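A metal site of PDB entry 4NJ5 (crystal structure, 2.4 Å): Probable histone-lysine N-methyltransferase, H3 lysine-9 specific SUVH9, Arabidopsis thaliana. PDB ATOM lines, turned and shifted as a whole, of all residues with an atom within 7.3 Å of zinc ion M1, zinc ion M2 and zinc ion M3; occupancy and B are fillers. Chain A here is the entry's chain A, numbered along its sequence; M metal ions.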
ATOM      1  N   SER A 300     -14.999 -18.080  20.247  1.00  0.00           N
ATOM      2  CA  SER A 300     -15.217 -16.648  20.359  1.00  0.00           C
ATOM      3  C   SER A 300     -14.177 -15.996  21.270  1.00  0.00           C
ATOM      4  O   SER A 300     -13.714 -16.617  22.231  1.00  0.00           O
ATOM      5  CB  SER A 300     -16.609 -16.411  20.896  1.00  0.00           C
ATOM      6  OG  SER A 300     -16.850 -17.317  21.945  1.00  0.00           O
ATOM      7  N   GLY A 301     -13.814 -14.757  20.960  1.00  0.00           N
ATOM      8  CA  GLY A 301     -12.835 -14.017  21.741  1.00  0.00           C
ATOM      9  C   GLY A 301     -13.470 -12.816  22.412  1.00  0.00           C
ATOM     10  O   GLY A 301     -14.583 -12.412  22.065  1.00  0.00           O
ATOM     11  N   CYS A 302     -12.768 -12.245  23.389  1.00  0.00           N
ATOM     12  CA  CYS A 302     -13.246 -11.033  24.028  1.00  0.00           C
ATOM     13  C   CYS A 302     -12.965  -9.818  23.142  1.00  0.00           C
ATOM     14  O   CYS A 302     -12.233  -9.912  22.146  1.00  0.00           O
ATOM     15  CB  CYS A 302     -12.632 -10.844  25.413  1.00  0.00           C
ATOM     16  SG  CYS A 302     -10.865 -10.551  25.390  1.00  0.00           S
ATOM     17  N   ASP A 303     -13.551  -8.685  23.503  1.00  0.00           N
ATOM     18  CA  ASP A 303     -13.447  -7.463  22.703  1.00  0.00           C
ATOM     19  C   ASP A 303     -12.728  -6.346  23.442  1.00  0.00           C
ATOM     20  O   ASP A 303     -13.072  -5.171  23.300  1.00  0.00           O
ATOM     21  CB  ASP A 303     -14.854  -6.994  22.294  1.00  0.00           C
ATOM     22  CG  ASP A 303     -15.764  -6.750  23.484  1.00  0.00           C
ATOM     23  OD1 ASP A 303     -15.336  -7.015  24.628  1.00  0.00           O
ATOM     24  OD2 ASP A 303     -16.909  -6.308  23.273  1.00  0.00           O
ATOM     25  N   CYS A 304     -11.721  -6.714  24.237  1.00  0.00           N
ATOM     26  CA  CYS A 304     -11.002  -5.767  25.077  1.00  0.00           C
ATOM     27  C   CYS A 304      -9.866  -5.069  24.345  1.00  0.00           C
ATOM     28  O   CYS A 304      -8.699  -5.334  24.614  1.00  0.00           O
ATOM     29  CB  CYS A 304     -10.458  -6.467  26.328  1.00  0.00           C
ATOM     30  SG  CYS A 304     -11.740  -7.228  27.332  1.00  0.00           S
ATOM     31  N   VAL A 305     -10.219  -4.164  23.444  1.00  0.00           N
ATOM     32  CA  VAL A 305      -9.258  -3.519  22.557  1.00  0.00           C
ATOM     33  C   VAL A 305      -8.147  -2.742  23.267  1.00  0.00           C
ATOM     34  O   VAL A 305      -7.152  -2.369  22.649  1.00  0.00           O
ATOM     35  CB  VAL A 305      -9.967  -2.602  21.551  1.00  0.00           C
ATOM     36  CG1 VAL A 305     -10.951  -3.408  20.717  1.00  0.00           C
ATOM     37  CG2 VAL A 305     -10.678  -1.472  22.276  1.00  0.00           C
ATOM     38  N   GLY A 307      -6.873  -4.124  26.252  1.00  0.00           N
ATOM     39  CA  GLY A 307      -6.392  -5.098  27.207  1.00  0.00           C
ATOM     40  C   GLY A 307      -7.495  -5.561  28.143  1.00  0.00           C
ATOM     41  O   GLY A 307      -8.381  -4.772  28.488  1.00  0.00           O
ATOM     42  N   CYS A 308      -7.455  -6.826  28.540  1.00  0.00           N
ATOM     43  CA  CYS A 308      -8.478  -7.357  29.437  1.00  0.00           C
ATOM     44  C   CYS A 308      -8.442  -6.666  30.789  1.00  0.00           C
ATOM     45  O   CYS A 308      -7.397  -6.581  31.424  1.00  0.00           O
ATOM     46  CB  CYS A 308      -8.330  -8.872  29.625  1.00  0.00           C
ATOM     47  SG  CYS A 308      -8.845  -9.855  28.204  1.00  0.00           S
ATOM     48  N   GLY A 309      -9.596  -6.170  31.210  1.00  0.00           N
ATOM     49  CA  GLY A 309      -9.756  -5.614  32.544  1.00  0.00           C
ATOM     50  C   GLY A 309     -10.685  -6.502  33.349  1.00  0.00           C
ATOM     51  O   GLY A 309     -10.297  -7.599  33.751  1.00  0.00           O
ATOM     52  N   SER A 310     -11.914  -6.049  33.553  1.00  0.00           N
ATOM     53  CA  SER A 310     -12.903  -6.798  34.324  1.00  0.00           C
ATOM     54  C   SER A 310     -14.227  -6.916  33.574  1.00  0.00           C
ATOM     55  O   SER A 310     -14.633  -5.996  32.866  1.00  0.00           O
ATOM     56  CB  SER A 310     -13.155  -6.136  35.675  1.00  0.00           C
ATOM     57  OG  SER A 310     -12.079  -6.374  36.574  1.00  0.00           O
ATOM     58  N   GLY A 311     -14.906  -8.049  33.740  1.00  0.00           N
ATOM     59  CA  GLY A 311     -16.242  -8.221  33.214  1.00  0.00           C
ATOM     60  C   GLY A 311     -16.350  -8.599  31.759  1.00  0.00           C
ATOM     61  O   GLY A 311     -17.416  -8.478  31.158  1.00  0.00           O
ATOM     62  N   CYS A 312     -15.248  -9.064  31.161  1.00  0.00           N
ATOM     63  CA  CYS A 312     -15.296  -9.507  29.773  1.00  0.00           C
ATOM     64  C   CYS A 312     -15.579 -11.009  29.676  1.00  0.00           C
ATOM     65  O   CYS A 312     -15.632 -11.714  30.687  1.00  0.00           O
ATOM     66  CB  CYS A 312     -14.008  -9.148  29.038  1.00  0.00           C
ATOM     67  SG  CYS A 312     -12.682 -10.374  29.155  1.00  0.00           S
ATOM     68  N   LEU A 313     -15.772 -11.478  28.443  1.00  0.00           N
ATOM     69  CA  LEU A 313     -16.101 -12.877  28.180  1.00  0.00           C
ATOM     70  C   LEU A 313     -15.016 -13.839  28.665  1.00  0.00           C
ATOM     71  O   LEU A 313     -15.317 -14.864  29.278  1.00  0.00           O
ATOM     72  CB  LEU A 313     -16.341 -13.075  26.670  1.00  0.00           C
ATOM     73  CG  LEU A 313     -15.971 -14.421  26.047  1.00  0.00           C
ATOM     74  CD1 LEU A 313     -16.950 -15.507  26.442  1.00  0.00           C
ATOM     75  CD2 LEU A 313     -15.856 -14.301  24.535  1.00  0.00           C
ATOM     76  N   CYS A 314     -13.762 -13.495  28.389  1.00  0.00           N
ATOM     77  CA  CYS A 314     -12.645 -14.337  28.793  1.00  0.00           C
ATOM     78  C   CYS A 314     -12.525 -14.466  30.311  1.00  0.00           C
ATOM     79  O   CYS A 314     -12.072 -15.492  30.815  1.00  0.00           O
ATOM     80  CB  CYS A 314     -11.346 -13.834  28.172  1.00  0.00           C
ATOM     81  SG  CYS A 314     -11.256 -14.137  26.394  1.00  0.00           S
ATOM     82  N   GLU A 315     -12.955 -13.437  31.042  1.00  0.00           N
ATOM     83  CA  GLU A 315     -13.020 -13.547  32.492  1.00  0.00           C
ATOM     84  C   GLU A 315     -14.083 -14.556  32.906  1.00  0.00           C
ATOM     85  O   GLU A 315     -13.885 -15.354  33.816  1.00  0.00           O
ATOM     86  CB  GLU A 315     -13.282 -12.191  33.144  1.00  0.00           C
ATOM     87  CG  GLU A 315     -13.447 -12.280  34.653  1.00  0.00           C
ATOM     88  CD  GLU A 315     -13.396 -10.931  35.346  1.00  0.00           C
ATOM     89  OE1 GLU A 315     -12.320 -10.561  35.841  1.00  0.00           O
ATOM     90  OE2 GLU A 315     -14.446 -10.240  35.396  1.00  0.00           O
ATOM     91  N   LYS A 317     -14.976 -17.064  31.164  1.00  0.00           N
ATOM     92  CA  LYS A 317     -14.406 -18.364  30.824  1.00  0.00           C
ATOM     93  C   LYS A 317     -13.507 -18.871  31.952  1.00  0.00           C
ATOM     94  O   LYS A 317     -13.341 -20.075  32.133  1.00  0.00           O
ATOM     95  CB  LYS A 317     -13.625 -18.307  29.504  1.00  0.00           C
ATOM     96  CG  LYS A 317     -14.452 -17.863  28.297  1.00  0.00           C
ATOM     97  CD  LYS A 317     -13.587 -17.752  27.027  1.00  0.00           C
ATOM     98  CE  LYS A 317     -13.203 -19.120  26.485  1.00  0.00           C
ATOM     99  NZ  LYS A 317     -11.974 -19.074  25.642  1.00  0.00           N
ATOM    100  N   ILE A 322      -9.685 -13.463  35.923  1.00  0.00           N
ATOM    101  CA  ILE A 322      -8.522 -13.560  35.047  1.00  0.00           C
ATOM    102  C   ILE A 322      -7.341 -14.095  35.846  1.00  0.00           C
ATOM    103  O   ILE A 322      -7.024 -13.599  36.918  1.00  0.00           O
ATOM    104  CB  ILE A 322      -8.155 -12.182  34.454  1.00  0.00           C
ATOM    105  CG1 ILE A 322      -9.325 -11.617  33.650  1.00  0.00           C
ATOM    106  CG2 ILE A 322      -6.925 -12.302  33.567  1.00  0.00           C
ATOM    107  CD1 ILE A 322      -9.542 -12.319  32.314  1.00  0.00           C
ATOM    108  N   HIS A 338      -7.782 -20.150  30.721  1.00  0.00           N
ATOM    109  CA  HIS A 338      -8.110 -19.733  29.356  1.00  0.00           C
ATOM    110  C   HIS A 338      -7.465 -18.383  29.050  1.00  0.00           C
ATOM    111  O   HIS A 338      -7.963 -17.337  29.475  1.00  0.00           O
ATOM    112  CB  HIS A 338      -9.630 -19.637  29.165  1.00  0.00           C
ATOM    113  CG  HIS A 338     -10.360 -20.924  29.380  1.00  0.00           C
ATOM    114  ND1 HIS A 338     -10.631 -21.810  28.351  1.00  0.00           N
ATOM    115  CD2 HIS A 338     -10.883 -21.479  30.498  1.00  0.00           C
ATOM    116  CE1 HIS A 338     -11.285 -22.848  28.831  1.00  0.00           C
ATOM    117  NE2 HIS A 338     -11.455 -22.679  30.127  1.00  0.00           N
ATOM    118  N   GLU A 339      -6.360 -18.408  28.331  1.00  0.00           N
ATOM    119  CA  GLU A 339      -5.718 -17.175  27.884  1.00  0.00           C
ATOM    120  C   GLU A 339      -6.416 -16.670  26.634  1.00  0.00           C
ATOM    121  O   GLU A 339      -7.103 -17.420  25.950  1.00  0.00           O
ATOM    122  CB  GLU A 339      -4.223 -17.395  27.612  1.00  0.00           C
ATOM    123  CG  GLU A 339      -3.383 -17.470  28.878  1.00  0.00           C
ATOM    124  CD  GLU A 339      -1.890 -17.549  28.601  1.00  0.00           C
ATOM    125  OE1 GLU A 339      -1.478 -17.338  27.440  1.00  0.00           O
ATOM    126  OE2 GLU A 339      -1.140 -17.817  29.569  1.00  0.00           O
ATOM    127  N   CYS A 340      -6.243 -15.382  26.336  1.00  0.00           N
ATOM    128  CA  CYS A 340      -6.790 -14.820  25.111  1.00  0.00           C
ATOM    129  C   CYS A 340      -6.057 -15.382  23.899  1.00  0.00           C
ATOM    130  O   CYS A 340      -4.857 -15.662  23.969  1.00  0.00           O
ATOM    131  CB  CYS A 340      -6.685 -13.300  25.129  1.00  0.00           C
ATOM    132  SG  CYS A 340      -7.606 -12.544  26.469  1.00  0.00           S
ATOM    133  N   GLY A 341      -6.786 -15.563  22.813  1.00  0.00           N
ATOM    134  CA  GLY A 341      -6.196 -16.072  21.583  1.00  0.00           C
ATOM    135  C   GLY A 341      -6.460 -15.163  20.397  1.00  0.00           C
ATOM    136  O   GLY A 341      -6.784 -13.982  20.568  1.00  0.00           O
ATOM    137  N   ALA A 343      -8.866 -15.053  18.402  1.00  0.00           N
ATOM    138  CA  ALA A 343     -10.247 -14.585  18.337  1.00  0.00           C
ATOM    139  C   ALA A 343     -10.472 -13.354  19.221  1.00  0.00           C
ATOM    140  O   ALA A 343     -11.433 -12.615  19.033  1.00  0.00           O
ATOM    141  CB  ALA A 343     -11.212 -15.703  18.712  1.00  0.00           C
ATOM    142  N   CYS A 344      -9.572 -13.126  20.176  1.00  0.00           N
ATOM    143  CA  CYS A 344      -9.673 -11.954  21.031  1.00  0.00           C
ATOM    144  C   CYS A 344      -9.112 -10.702  20.373  1.00  0.00           C
ATOM    145  O   CYS A 344      -8.181 -10.772  19.560  1.00  0.00           O
ATOM    146  CB  CYS A 344      -8.992 -12.204  22.380  1.00  0.00           C
ATOM    147  SG  CYS A 344      -9.722 -13.569  23.310  1.00  0.00           S
ATOM    148  N   GLN A 345      -9.680  -9.552  20.718  1.00  0.00           N
ATOM    149  CA  GLN A 345      -9.317  -8.289  20.087  1.00  0.00           C
ATOM    150  C   GLN A 345      -8.366  -7.478  20.958  1.00  0.00           C
ATOM    151  O   GLN A 345      -8.008  -6.353  20.610  1.00  0.00           O
ATOM    152  CB  GLN A 345     -10.568  -7.486  19.745  1.00  0.00           C
ATOM    153  CG  GLN A 345     -11.415  -8.134  18.672  1.00  0.00           C
ATOM    154  CD  GLN A 345     -12.771  -7.475  18.520  1.00  0.00           C
ATOM    155  OE1 GLN A 345     -13.614  -7.550  19.413  1.00  0.00           O
ATOM    156  NE2 GLN A 345     -13.000  -6.833  17.387  1.00  0.00           N
ATOM    157  N   CYS A 346      -7.960  -8.046  22.088  1.00  0.00           N
ATOM    158  CA  CYS A 346      -6.955  -7.412  22.927  1.00  0.00           C
ATOM    159  C   CYS A 346      -5.590  -7.512  22.257  1.00  0.00           C
ATOM    160  O   CYS A 346      -5.330  -8.465  21.520  1.00  0.00           O
ATOM    161  CB  CYS A 346      -6.939  -8.035  24.325  1.00  0.00           C
ATOM    162  SG  CYS A 346      -6.858  -9.828  24.352  1.00  0.00           S
ATOM    163  N   PRO A 347      -4.718  -6.519  22.498  1.00  0.00           N
ATOM    164  CA  PRO A 347      -3.352  -6.494  21.958  1.00  0.00           C
ATOM    165  C   PRO A 347      -2.453  -7.479  22.698  1.00  0.00           C
ATOM    166  O   PRO A 347      -2.879  -8.061  23.697  1.00  0.00           O
ATOM    167  CB  PRO A 347      -2.914  -5.056  22.247  1.00  0.00           C
ATOM    168  CG  PRO A 347      -3.689  -4.663  23.455  1.00  0.00           C
ATOM    169  CD  PRO A 347      -5.026  -5.308  23.278  1.00  0.00           C
ATOM    170  N   SER A 349      -0.128  -6.916  24.646  1.00  0.00           N
ATOM    171  CA  SER A 349       0.190  -6.447  25.998  1.00  0.00           C
ATOM    172  C   SER A 349      -0.868  -6.819  27.038  1.00  0.00           C
ATOM    173  O   SER A 349      -0.686  -6.556  28.224  1.00  0.00           O
ATOM    174  CB  SER A 349       0.384  -4.923  25.998  1.00  0.00           C
ATOM    175  OG  SER A 349      -0.859  -4.268  25.854  1.00  0.00           O
ATOM    176  N   CYS A 350      -1.968  -7.414  26.593  1.00  0.00           N
ATOM    177  CA  CYS A 350      -3.032  -7.831  27.506  1.00  0.00           C
ATOM    178  C   CYS A 350      -2.521  -8.769  28.605  1.00  0.00           C
ATOM    179  O   CYS A 350      -1.729  -9.676  28.342  1.00  0.00           O
ATOM    180  CB  CYS A 350      -4.166  -8.501  26.749  1.00  0.00           C
ATOM    181  SG  CYS A 350      -5.364  -9.306  27.833  1.00  0.00           S
ATOM    182  N   ARG A 351      -2.989  -8.558  29.823  1.00  0.00           N
ATOM    183  CA  ARG A 351      -2.542  -9.358  30.970  1.00  0.00           C
ATOM    184  C   ARG A 351      -2.963 -10.823  30.886  1.00  0.00           C
ATOM    185  O   ARG A 351      -2.481 -11.659  31.641  1.00  0.00           O
ATOM    186  CB  ARG A 351      -3.049  -8.751  32.286  1.00  0.00           C
ATOM    187  CG  ARG A 351      -4.545  -8.929  32.520  1.00  0.00           C
ATOM    188  CD  ARG A 351      -4.954  -8.390  33.886  1.00  0.00           C
ATOM    189  NE  ARG A 351      -6.401  -8.280  34.017  1.00  0.00           N
ATOM    190  CZ  ARG A 351      -7.106  -8.845  34.988  1.00  0.00           C
ATOM    191  NH1 ARG A 351      -6.511  -9.564  35.923  1.00  0.00           N
ATOM    192  NH2 ARG A 351      -8.423  -8.678  35.036  1.00  0.00           N
ATOM    193  N   ASN A 352      -3.871 -11.147  29.974  1.00  0.00           N
ATOM    194  CA  ASN A 352      -4.328 -12.526  29.836  1.00  0.00           C
ATOM    195  C   ASN A 352      -3.621 -13.260  28.700  1.00  0.00           C
ATOM    196  O   ASN A 352      -4.194 -14.158  28.071  1.00  0.00           O
ATOM    197  CB  ASN A 352      -5.852 -12.588  29.674  1.00  0.00           C
ATOM    198  CG  ASN A 352      -6.413 -13.943  30.047  1.00  0.00           C
ATOM    199  OD1 ASN A 352      -5.855 -14.641  30.894  1.00  0.00           O
ATOM    200  ND2 ASN A 352      -7.516 -14.318  29.414  1.00  0.00           N
ATOM    201  N   ARG A 353      -2.374 -12.876  28.431  1.00  0.00           N
ATOM    202  CA  ARG A 353      -1.571 -13.521  27.399  1.00  0.00           C
ATOM    203  C   ARG A 353      -0.179 -13.877  27.911  1.00  0.00           C
ATOM    204  O   ARG A 353       0.818 -13.641  27.236  1.00  0.00           O
ATOM    205  CB  ARG A 353      -1.458 -12.612  26.160  1.00  0.00           C
ATOM    206  CG  ARG A 353      -2.758 -12.358  25.416  1.00  0.00           C
ATOM    207  CD  ARG A 353      -2.523 -11.548  24.152  1.00  0.00           C
ATOM    208  NE  ARG A 353      -3.754 -11.223  23.428  1.00  0.00           N
ATOM    209  CZ  ARG A 353      -4.296 -11.987  22.491  1.00  0.00           C
ATOM    210  NH1 ARG A 353      -3.734 -13.145  22.168  1.00  0.00           N
ATOM    211  NH2 ARG A 353      -5.410 -11.613  21.882  1.00  0.00           N
HETATM  212 ZN    ZN M   1     -11.032  -9.392  27.664  1.00  0.00          ZN
HETATM  213 ZN    ZN M   2      -9.776 -12.600  25.542  1.00  0.00          ZN
HETATM  214 ZN    ZN M   3      -7.207 -10.182  26.634  1.00  0.00          ZN
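Zinc ion M1 is bound by the side-chain sulfur of Cys 308 (2.3 Å), the side-chain sulfur of Cys 304 (2.3 Å), the side-chain sulfur of Cys 312 (2.4 Å) and the side-chain sulfur of Cys 302 (2.6 Å).
Zinc ion M1 has four donor atoms within binding distance.
The backbone NH of Cys 314 sits close to the side-chain sulfur of Cys 312, at 3.4 Å.
The backbone carbonyl oxygen (O) of Cys 302 is in hydrogen-bond range of the backbone NH (N) of Gln 345.
The backbone carbonyl oxygen (O) of Cys 346 sits at hydrogen-bond distance from the guanidinium group (NH2) of Arg 353, 3.2 Å away.
O of Asn 352 sits at hydrogen-bond distance from N of Cys 340, 3.0 Å away.
The backbone carbonyl oxygen (O) of Cys 340 lies within hydrogen-bond range of the guanidinium group (NH1) of Arg 353.
The backbone NH (N) of Asn 352 sits close to the side-chain sulfur (SG) of Cys 350.
SG of Cys 312 sits close to N of Glu 315 (3.6 Å).
SG of Cys 344 lies close to N of Gly 341 (3.6 Å).
Of the 31 residues printed, 5 come within 4 Å of zinc ion M2.
The nearest printed residue that does not touch zinc ion M2 is Cys 346 (4.2 Å).
Zinc ion M2 is bound by SG of Cys 314, 2.3 Å away.
Zinc ion M2 is bound by the side-chain sulfur (SG) of Cys 302 (2.3 Å).
The side-chain sulfur (SG) of Cys 340 binds zinc ion M2 (2.4 Å).
Zinc ion M2 is bound by the side-chain sulfur (SG) of Cys 344 (2.4 Å).
Zinc ion M2 has four donor atoms within binding distance.
Four residues have an atom within 4 Å of zinc ion M1: Cys 302, Cys 304, Cys 308 and Cys 312.
Along chain A the residues within 4 Å of zinc ion M1 span positions 302 to 312.
The nearest printed residue that does not touch zinc ion M1 is Cys 314 (4.5 Å).
SG of Cys 308 binds zinc ion M3, at 2.3 Å.
SG of Cys 346 is bound to zinc ion M3, 2.3 Å away.
SG of Cys 350 is bound to zinc ion M3 (2.4 Å).
SG of Cys 340 binds zinc ion M3, at 2.4 Å.
Zinc ion M3 has four donor atoms within binding distance.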
